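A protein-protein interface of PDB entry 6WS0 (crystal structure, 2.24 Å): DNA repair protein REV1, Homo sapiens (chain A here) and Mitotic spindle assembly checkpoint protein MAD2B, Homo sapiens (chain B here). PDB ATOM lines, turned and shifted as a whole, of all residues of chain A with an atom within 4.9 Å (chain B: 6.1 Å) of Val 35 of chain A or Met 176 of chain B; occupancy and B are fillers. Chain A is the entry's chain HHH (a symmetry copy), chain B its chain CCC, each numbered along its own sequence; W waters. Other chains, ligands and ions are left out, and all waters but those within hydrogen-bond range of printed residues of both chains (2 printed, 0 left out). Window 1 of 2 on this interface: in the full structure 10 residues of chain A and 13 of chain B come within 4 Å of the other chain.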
ATOM      1  N   ILE A  31      -4.437 -30.825 -20.694  1.00  0.00           N
ATOM      2  CA  ILE A  31      -4.277 -29.379 -20.412  1.00  0.00           C
ATOM      3  C   ILE A  31      -2.873 -29.159 -19.818  1.00  0.00           C
ATOM      4  O   ILE A  31      -2.197 -28.218 -20.274  1.00  0.00           O
ATOM      5  CB  ILE A  31      -5.418 -28.854 -19.534  1.00  0.00           C
ATOM      6  CG1 ILE A  31      -6.777 -29.057 -20.209  1.00  0.00           C
ATOM      7  CG2 ILE A  31      -5.176 -27.389 -19.172  1.00  0.00           C
ATOM      8  CD1 ILE A  31      -7.916 -28.825 -19.249  1.00  0.00           C
ATOM      9  N   LEU A  32      -2.418 -30.022 -18.904  1.00  0.00           N
ATOM     10  CA  LEU A  32      -1.115 -29.854 -18.198  1.00  0.00           C
ATOM     11  C   LEU A  32       0.017 -30.024 -19.212  1.00  0.00           C
ATOM     12  O   LEU A  32       1.014 -29.267 -19.145  1.00  0.00           O
ATOM     13  CB  LEU A  32      -1.016 -30.851 -17.040  1.00  0.00           C
ATOM     14  CG  LEU A  32      -1.894 -30.496 -15.844  1.00  0.00           C
ATOM     15  CD1 LEU A  32      -1.584 -31.381 -14.660  1.00  0.00           C
ATOM     16  CD2 LEU A  32      -1.701 -29.054 -15.440  1.00  0.00           C
ATOM     17  N   GLN A  33      -0.163 -30.977 -20.125  1.00  0.00           N
ATOM     18  CA  GLN A  33       0.755 -31.252 -21.249  1.00  0.00           C
ATOM     19  C   GLN A  33       0.876 -29.979 -22.106  1.00  0.00           C
ATOM     20  O   GLN A  33       1.947 -29.727 -22.647  1.00  0.00           O
ATOM     21  CB  GLN A  33       0.218 -32.454 -22.029  1.00  0.00           C
ATOM     22  CG  GLN A  33       1.281 -33.469 -22.423  1.00  0.00           C
ATOM     23  CD  GLN A  33       1.653 -34.361 -21.269  1.00  0.00           C
ATOM     24  OE1 GLN A  33       0.788 -34.946 -20.620  1.00  0.00           O
ATOM     25  NE2 GLN A  33       2.946 -34.446 -20.990  1.00  0.00           N
ATOM     26  N   VAL A  34      -0.178 -29.184 -22.282  1.00  0.00           N
ATOM     27  CA  VAL A  34      -0.024 -27.959 -23.112  1.00  0.00           C
ATOM     28  C   VAL A  34       0.708 -26.925 -22.269  1.00  0.00           C
ATOM     29  O   VAL A  34       1.556 -26.200 -22.802  1.00  0.00           O
ATOM     30  CB  VAL A  34      -1.372 -27.426 -23.619  1.00  0.00           C
ATOM     31  CG1 VAL A  34      -1.251 -26.003 -24.138  1.00  0.00           C
ATOM     32  CG2 VAL A  34      -1.957 -28.375 -24.663  1.00  0.00           C
ATOM     33  N   VAL A  35       0.401 -26.830 -20.981  1.00  0.00           N
ATOM     34  CA  VAL A  35       1.197 -25.890 -20.158  1.00  0.00           C
ATOM     35  C   VAL A  35       2.702 -26.231 -20.236  1.00  0.00           C
ATOM     36  O   VAL A  35       3.481 -25.307 -20.389  1.00  0.00           O
ATOM     37  CB  VAL A  35       0.717 -25.862 -18.708  1.00  0.00           C
ATOM     38  CG1 VAL A  35       1.748 -25.098 -17.886  1.00  0.00           C
ATOM     39  CG2 VAL A  35      -0.685 -25.262 -18.620  1.00  0.00           C
ATOM     40  N   LYS A  36       3.098 -27.490 -20.068  1.00  0.00           N
ATOM     41  CA  LYS A  36       4.520 -27.939 -20.094  1.00  0.00           C
ATOM     42  C   LYS A  36       5.136 -27.682 -21.477  1.00  0.00           C
ATOM     43  O   LYS A  36       6.276 -27.125 -21.563  1.00  0.00           O
ATOM     44  CB  LYS A  36       4.584 -29.427 -19.767  1.00  0.00           C
ATOM     45  CG  LYS A  36       5.873 -30.134 -20.163  1.00  0.00           C
ATOM     46  CD  LYS A  36       6.708 -30.656 -19.024  1.00  0.00           C
ATOM     47  CE  LYS A  36       7.662 -31.749 -19.472  1.00  0.00           C
ATOM     48  NZ  LYS A  36       8.637 -31.273 -20.485  1.00  0.00           N
ATOM     49  N   TYR A  37       4.408 -28.025 -22.541  1.00  0.00           N
ATOM     50  CA  TYR A  37       4.753 -27.587 -23.911  1.00  0.00           C
ATOM     51  C   TYR A  37       5.044 -26.074 -23.886  1.00  0.00           C
ATOM     52  O   TYR A  37       6.124 -25.645 -24.260  1.00  0.00           O
ATOM     53  CB  TYR A  37       3.677 -27.941 -24.942  1.00  0.00           C
ATOM     54  CG  TYR A  37       4.046 -27.469 -26.328  1.00  0.00           C
ATOM     55  CD1 TYR A  37       5.089 -28.062 -27.018  1.00  0.00           C
ATOM     56  CD2 TYR A  37       3.389 -26.407 -26.934  1.00  0.00           C
ATOM     57  CE1 TYR A  37       5.471 -27.619 -28.275  1.00  0.00           C
ATOM     58  CE2 TYR A  37       3.736 -25.969 -28.202  1.00  0.00           C
ATOM     59  CZ  TYR A  37       4.797 -26.566 -28.860  1.00  0.00           C
ATOM     60  OH  TYR A  37       5.177 -26.123 -30.087  1.00  0.00           O
ATOM     61  N   CYS A  38       4.134 -25.237 -23.418  1.00  0.00           N
ATOM     62  CA  CYS A  38       4.379 -23.763 -23.450  1.00  0.00           C
ATOM     63  C   CYS A  38       5.606 -23.366 -22.606  1.00  0.00           C
ATOM     64  O   CYS A  38       6.394 -22.525 -23.047  1.00  0.00           O
ATOM     65  CB  CYS A  38       3.143 -23.001 -23.014  1.00  0.00           C
ATOM     66  SG  CYS A  38       1.825 -23.099 -24.244  1.00  0.00           S
ATOM     67  N   THR A  39       5.789 -23.908 -21.410  1.00  0.00           N
ATOM     68  CA  THR A  39       6.941 -23.500 -20.548  1.00  0.00           C
ATOM     69  C   THR A  39       8.252 -24.005 -21.169  1.00  0.00           C
ATOM     70  O   THR A  39       9.272 -23.320 -21.004  1.00  0.00           O
ATOM     71  CB  THR A  39       6.698 -23.914 -19.095  1.00  0.00           C
ATOM     72  OG1 THR A  39       6.415 -25.298 -19.032  1.00  0.00           O
ATOM     73  CG2 THR A  39       5.503 -23.206 -18.497  1.00  0.00           C
ATOM     74  N   PHE A  75      -6.401 -20.917 -17.665  1.00  0.00           N
ATOM     75  CA  PHE A  75      -5.541 -21.699 -16.759  1.00  0.00           C
ATOM     76  C   PHE A  75      -4.147 -21.774 -17.410  1.00  0.00           C
ATOM     77  O   PHE A  75      -3.142 -21.407 -16.793  1.00  0.00           O
ATOM     78  CB  PHE A  75      -6.196 -23.047 -16.446  1.00  0.00           C
ATOM     79  CG  PHE A  75      -5.229 -23.975 -15.767  1.00  0.00           C
ATOM     80  CD1 PHE A  75      -5.062 -23.955 -14.385  1.00  0.00           C
ATOM     81  CD2 PHE A  75      -4.426 -24.798 -16.525  1.00  0.00           C
ATOM     82  CE1 PHE A  75      -4.105 -24.759 -13.780  1.00  0.00           C
ATOM     83  CE2 PHE A  75      -3.516 -25.638 -15.905  1.00  0.00           C
ATOM     84  CZ  PHE A  75      -3.341 -25.609 -14.543  1.00  0.00           C
ATOM     85  N   ILE A  76      -4.117 -22.142 -18.684  1.00  0.00           N
ATOM     86  CA  ILE A  76      -2.876 -22.267 -19.474  1.00  0.00           C
ATOM     87  C   ILE A  76      -2.110 -20.953 -19.436  1.00  0.00           C
ATOM     88  O   ILE A  76      -0.920 -20.937 -19.062  1.00  0.00           O
ATOM     89  CB  ILE A  76      -3.174 -22.738 -20.900  1.00  0.00           C
ATOM     90  CG1 ILE A  76      -3.636 -24.198 -20.907  1.00  0.00           C
ATOM     91  CG2 ILE A  76      -1.943 -22.555 -21.758  1.00  0.00           C
ATOM     92  CD1 ILE A  76      -4.239 -24.659 -22.229  1.00  0.00           C
ATOM     93  N   ASN A  79      -0.455 -19.928 -16.064  1.00  0.00           N
ATOM     94  CA  ASN A  79       0.758 -20.695 -15.705  1.00  0.00           C
ATOM     95  C   ASN A  79       1.895 -20.304 -16.649  1.00  0.00           C
ATOM     96  O   ASN A  79       3.051 -20.514 -16.209  1.00  0.00           O
ATOM     97  CB  ASN A  79       0.487 -22.195 -15.608  1.00  0.00           C
ATOM     98  CG  ASN A  79      -0.351 -22.450 -14.381  1.00  0.00           C
ATOM     99  OD1 ASN A  79       0.168 -22.383 -13.292  1.00  0.00           O
ATOM    100  ND2 ASN A  79      -1.648 -22.681 -14.531  1.00  0.00           N
ATOM    101  N   VAL A  80       1.603 -19.744 -17.835  1.00  0.00           N
ATOM    102  CA  VAL A  80       2.680 -19.239 -18.741  1.00  0.00           C
ATOM    103  C   VAL A  80       3.115 -17.863 -18.212  1.00  0.00           C
ATOM    104  O   VAL A  80       4.328 -17.628 -18.096  1.00  0.00           O
ATOM    105  CB  VAL A  80       2.307 -19.204 -20.248  1.00  0.00           C
ATOM    106  CG1 VAL A  80       3.195 -18.244 -21.053  1.00  0.00           C
ATOM    107  CG2 VAL A  80       2.369 -20.593 -20.899  1.00  0.00           C
ATOM    108  N   LEU B  90      -1.721 -28.953  -1.246  1.00  0.00           N
ATOM    109  CA  LEU B  90      -1.832 -30.211  -2.023  1.00  0.00           C
ATOM    110  C   LEU B  90      -1.848 -31.356  -0.999  1.00  0.00           C
ATOM    111  O   LEU B  90      -2.684 -32.295  -1.106  1.00  0.00           O
ATOM    112  CB  LEU B  90      -0.683 -30.277  -3.028  1.00  0.00           C
ATOM    113  CG  LEU B  90      -0.881 -29.509  -4.334  1.00  0.00           C
ATOM    114  CD1 LEU B  90      -1.105 -28.035  -4.064  1.00  0.00           C
ATOM    115  CD2 LEU B  90       0.331 -29.676  -5.237  1.00  0.00           C
ATOM    116  N   ALA B 172      -3.635 -33.031 -12.114  1.00  0.00           N
ATOM    117  CA  ALA B 172      -4.901 -32.300 -11.906  1.00  0.00           C
ATOM    118  C   ALA B 172      -4.623 -30.798 -11.901  1.00  0.00           C
ATOM    119  O   ALA B 172      -3.692 -30.345 -11.243  1.00  0.00           O
ATOM    120  CB  ALA B 172      -5.603 -32.750 -10.646  1.00  0.00           C
ATOM    121  N   THR B 173      -5.390 -30.111 -12.733  1.00  0.00           N
ATOM    122  CA  THR B 173      -5.507 -28.641 -12.857  1.00  0.00           C
ATOM    123  C   THR B 173      -5.487 -28.057 -11.448  1.00  0.00           C
ATOM    124  O   THR B 173      -4.677 -27.154 -11.232  1.00  0.00           O
ATOM    125  CB  THR B 173      -6.710 -28.342 -13.768  1.00  0.00           C
ATOM    126  OG1 THR B 173      -6.166 -28.442 -15.089  1.00  0.00           O
ATOM    127  CG2 THR B 173      -7.325 -26.980 -13.577  1.00  0.00           C
ATOM    128  N   ARG B 174      -6.232 -28.649 -10.513  1.00  0.00           N
ATOM    129  CA  ARG B 174      -6.394 -28.089  -9.149  1.00  0.00           C
ATOM    130  C   ARG B 174      -5.013 -28.046  -8.478  1.00  0.00           C
ATOM    131  O   ARG B 174      -4.741 -27.084  -7.763  1.00  0.00           O
ATOM    132  CB  ARG B 174      -7.429 -28.860  -8.321  1.00  0.00           C
ATOM    133  CG  ARG B 174      -6.878 -30.085  -7.580  1.00  0.00           C
ATOM    134  CD  ARG B 174      -7.937 -31.011  -6.943  1.00  0.00           C
ATOM    135  NE  ARG B 174      -7.447 -32.375  -6.729  1.00  0.00           N
ATOM    136  CZ  ARG B 174      -7.543 -33.382  -7.597  1.00  0.00           C
ATOM    137  NH1 ARG B 174      -8.168 -33.233  -8.758  1.00  0.00           N
ATOM    138  NH2 ARG B 174      -7.009 -34.553  -7.299  1.00  0.00           N
ATOM    139  N   ASN B 175      -4.152 -29.025  -8.726  1.00  0.00           N
ATOM    140  CA  ASN B 175      -2.824 -29.069  -8.070  1.00  0.00           C
ATOM    141  C   ASN B 175      -2.058 -27.766  -8.323  1.00  0.00           C
ATOM    142  O   ASN B 175      -1.490 -27.212  -7.388  1.00  0.00           O
ATOM    143  CB  ASN B 175      -2.012 -30.286  -8.521  1.00  0.00           C
ATOM    144  CG  ASN B 175      -2.542 -31.538  -7.866  1.00  0.00           C
ATOM    145  OD1 ASN B 175      -3.064 -31.447  -6.756  1.00  0.00           O
ATOM    146  ND2 ASN B 175      -2.458 -32.668  -8.559  1.00  0.00           N
ATOM    147  N   MET B 176      -2.046 -27.320  -9.558  1.00  0.00           N
ATOM    148  CA  MET B 176      -1.204 -26.202 -10.029  1.00  0.00           C
ATOM    149  C   MET B 176      -1.882 -24.860  -9.717  1.00  0.00           C
ATOM    150  O   MET B 176      -1.180 -23.931  -9.343  1.00  0.00           O
ATOM    151  CB  MET B 176      -1.037 -26.429 -11.520  1.00  0.00           C
ATOM    152  CG  MET B 176      -0.043 -25.595 -12.172  1.00  0.00           C
ATOM    153  SD  MET B 176       0.643 -26.613 -13.482  1.00  0.00           S
ATOM    154  CE  MET B 176       1.957 -25.484 -13.928  1.00  0.00           C
ATOM    155  N   GLU B 177      -3.213 -24.783  -9.782  1.00  0.00           N
ATOM    156  CA  GLU B 177      -3.997 -23.643  -9.236  1.00  0.00           C
ATOM    157  C   GLU B 177      -3.596 -23.399  -7.772  1.00  0.00           C
ATOM    158  O   GLU B 177      -3.398 -22.266  -7.376  1.00  0.00           O
ATOM    159  CB  GLU B 177      -5.498 -23.933  -9.372  1.00  0.00           C
ATOM    160  CG  GLU B 177      -5.974 -24.021 -10.824  1.00  0.00           C
ATOM    161  CD  GLU B 177      -7.467 -24.239 -11.041  1.00  0.00           C
ATOM    162  OE1 GLU B 177      -8.006 -25.251 -10.502  1.00  0.00           O
ATOM    163  OE2 GLU B 177      -8.087 -23.403 -11.760  1.00  0.00           O
ATOM    164  N   LYS B 178      -3.416 -24.444  -6.977  1.00  0.00           N
ATOM    165  CA  LYS B 178      -3.178 -24.263  -5.524  1.00  0.00           C
ATOM    166  C   LYS B 178      -1.723 -23.864  -5.278  1.00  0.00           C
ATOM    167  O   LYS B 178      -1.481 -23.132  -4.293  1.00  0.00           O
ATOM    168  CB  LYS B 178      -3.687 -25.506  -4.797  1.00  0.00           C
ATOM    169  CG  LYS B 178      -5.206 -25.653  -4.844  1.00  0.00           C
ATOM    170  CD  LYS B 178      -5.735 -27.056  -4.599  1.00  0.00           C
ATOM    171  CE  LYS B 178      -5.581 -27.500  -3.158  1.00  0.00           C
ATOM    172  NZ  LYS B 178      -6.880 -27.846  -2.535  1.00  0.00           N
ATOM    173  N   ILE B 179      -0.788 -24.232  -6.169  1.00  0.00           N
ATOM    174  CA  ILE B 179       0.672 -24.155  -5.856  1.00  0.00           C
ATOM    175  C   ILE B 179       1.261 -22.800  -6.271  1.00  0.00           C
ATOM    176  O   ILE B 179       2.341 -22.504  -5.793  1.00  0.00           O
ATOM    177  CB  ILE B 179       1.432 -25.318  -6.504  1.00  0.00           C
ATOM    178  CG1 ILE B 179       2.699 -25.660  -5.719  1.00  0.00           C
ATOM    179  CG2 ILE B 179       1.687 -24.983  -7.958  1.00  0.00           C
ATOM    180  CD1 ILE B 179       3.391 -26.976  -6.091  1.00  0.00           C
ATOM    181  N   GLN B 180       0.596 -22.023  -7.144  1.00  0.00           N
ATOM    182  CA  GLN B 180       1.055 -20.707  -7.689  1.00  0.00           C
ATOM    183  C   GLN B 180       0.458 -19.564  -6.861  1.00  0.00           C
ATOM    184  O   GLN B 180      -0.308 -18.803  -7.446  1.00  0.00           O
ATOM    185  CB  GLN B 180       0.566 -20.432  -9.125  1.00  0.00           C
ATOM    186  CG  GLN B 180       0.900 -21.479 -10.177  1.00  0.00           C
ATOM    187  CD  GLN B 180       2.356 -21.604 -10.569  1.00  0.00           C
ATOM    188  OE1 GLN B 180       3.268 -21.169  -9.861  1.00  0.00           O
ATOM    189  NE2 GLN B 180       2.583 -22.285 -11.690  1.00  0.00           N
ATOM    190  N   TRP B 187       5.835 -22.188 -10.012  1.00  0.00           N
ATOM    191  CA  TRP B 187       6.167 -23.601 -10.277  1.00  0.00           C
ATOM    192  C   TRP B 187       5.983 -23.909 -11.780  1.00  0.00           C
ATOM    193  O   TRP B 187       5.206 -23.186 -12.498  1.00  0.00           O
ATOM    194  CB  TRP B 187       5.292 -24.464  -9.392  1.00  0.00           C
ATOM    195  CG  TRP B 187       5.607 -24.354  -7.932  1.00  0.00           C
ATOM    196  CD1 TRP B 187       5.374 -23.281  -7.122  1.00  0.00           C
ATOM    197  CD2 TRP B 187       6.122 -25.386  -7.072  1.00  0.00           C
ATOM    198  NE1 TRP B 187       5.730 -23.553  -5.830  1.00  0.00           N
ATOM    199  CE2 TRP B 187       6.164 -24.852  -5.762  1.00  0.00           C
ATOM    200  CE3 TRP B 187       6.507 -26.718  -7.269  1.00  0.00           C
ATOM    201  CZ2 TRP B 187       6.576 -25.599  -4.667  1.00  0.00           C
ATOM    202  CZ3 TRP B 187       6.922 -27.453  -6.189  1.00  0.00           C
ATOM    203  CH2 TRP B 187       6.957 -26.898  -4.905  1.00  0.00           C
ATOM    204  N   ILE B 188       6.688 -24.943 -12.225  1.00  0.00           N
ATOM    205  CA  ILE B 188       6.608 -25.538 -13.575  1.00  0.00           C
ATOM    206  C   ILE B 188       6.456 -27.056 -13.470  1.00  0.00           C
ATOM    207  O   ILE B 188       6.799 -27.640 -12.445  1.00  0.00           O
ATOM    208  CB  ILE B 188       7.873 -25.173 -14.344  1.00  0.00           C
ATOM    209  CG1 ILE B 188       9.107 -25.651 -13.582  1.00  0.00           C
ATOM    210  CG2 ILE B 188       7.884 -23.684 -14.619  1.00  0.00           C
ATOM    211  CD1 ILE B 188      10.322 -25.724 -14.423  1.00  0.00           C
ATOM    212  N   LEU B 189       6.030 -27.679 -14.550  1.00  0.00           N
ATOM    213  CA  LEU B 189       6.024 -29.153 -14.686  1.00  0.00           C
ATOM    214  C   LEU B 189       7.440 -29.570 -15.054  1.00  0.00           C
ATOM    215  O   LEU B 189       7.999 -28.976 -15.971  1.00  0.00           O
ATOM    216  CB  LEU B 189       4.982 -29.503 -15.735  1.00  0.00           C
ATOM    217  CG  LEU B 189       3.575 -29.089 -15.323  1.00  0.00           C
ATOM    218  CD1 LEU B 189       2.652 -28.916 -16.524  1.00  0.00           C
ATOM    219  CD2 LEU B 189       3.005 -30.123 -14.387  1.00  0.00           C
HETATM  220  O   HOH W   1       3.899 -23.282 -15.084  1.00  0.00           O
HETATM  221  O   HOH W   2       4.964 -25.677 -16.433  1.00  0.00           O
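OD1 of Asn 79 of chain A sits at hydrogen-bond distance from NE2 of Gln 180 of chain B (2.9 Å).
O of Val 35 of chain A sits at hydrogen-bond distance from OG1 of Thr 39 of chain A, at 3.2 Å. The backbone carbonyl oxygen (O) of Lys 36 of chain A is in hydrogen-bond range of the side-chain hydroxyl (OG1) of Thr 39 of chain A, at 3.1 Å. The backbone carbonyl oxygen (O) of Phe 75 of chain A lies within hydrogen-bond range of the side-chain amide nitrogen (ND2) of Asn 79 of chain A (3.0 Å). The backbone NH of Trp 187 of chain B lies within hydrogen-bond range of the side-chain amide oxygen of Gln 180 of chain B (2.8 Å).
Leu 32 of chain A touches Ala 172 of chain B. Leu 32 of chain A touches Met 176 of chain B (CD2 to SD, 3.9 Å). Leu 32 of chain A touches Leu 189 of chain B. Met 176 of chain B touches Val 35 of chain A (CE to CG1, 3.98 Å). Lys 36 of chain A touches Leu 189 of chain B (CD to O, 3.7 Å). Phe 75 of chain A touches Thr 173 of chain B. Met 176 of chain B touches Phe 75 of chain A. CE1 of Phe 75 of chain A touches CG of Glu 177 of chain B, 3.6 Å away. Met 176 of chain B touches Asn 79 of chain A.
Of the printed residues of chain B, Val 35 of chain A touches Met 176. Of the printed residues of chain A, Met 176 of chain B touches Leu 32 (3.9 Å), Val 35 (3.98 Å), Phe 75 (3.9 Å) and Asn 79 (3.4 Å). Printed residues of chain B within 4 Å of Lys 36 of chain A: Leu 189. Of the printed residues of chain B, Asn 79 of chain A touches Met 176 (3.4 Å) and Gln 180 (2.9 Å). Printed residues of chain B within 4 Å of Phe 75 of chain A: Thr 173 (3.5 Å), Met 176 (3.9 Å) and Glu 177 (3.6 Å). Asn 175 of chain B touches none of the printed residues of chain A. Ile 179 of chain B touches none of the printed residues of chain A.
Of the 13 printed residues of chain B, 6 touch a printed residue of chain A. Hydrophobic or aromatic side chains of chain B that line the printed part of chain A: Met 176 and Leu 189. Of the 13 printed residues of chain A, 5 touch a printed residue of chain B. Printed residues of chain A that touch a printed residue of chain B: Leu 32, Val 35, Lys 36, Phe 75 and Asn 79. Hydrophobic or aromatic side chains of chain A that line the printed part of chain B: Leu 32, Val 35 and Phe 75. Among the printed residues, 10 pairs touch across the chains. Among the printed residues, no Asp or Glu carboxylate lies within 4 Å of a Lys or Arg side-chain nitrogen of the other chain.
Water W1 lies within hydrogen-bond range of the backbone carbonyl oxygen (O) of Trp 187 of chain B and the backbone carbonyl oxygen (O) of Asn 79 of chain A. Water W2 lies within hydrogen-bond range of N of Leu 189 of chain B and OG1 of Thr 39 of chain A.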
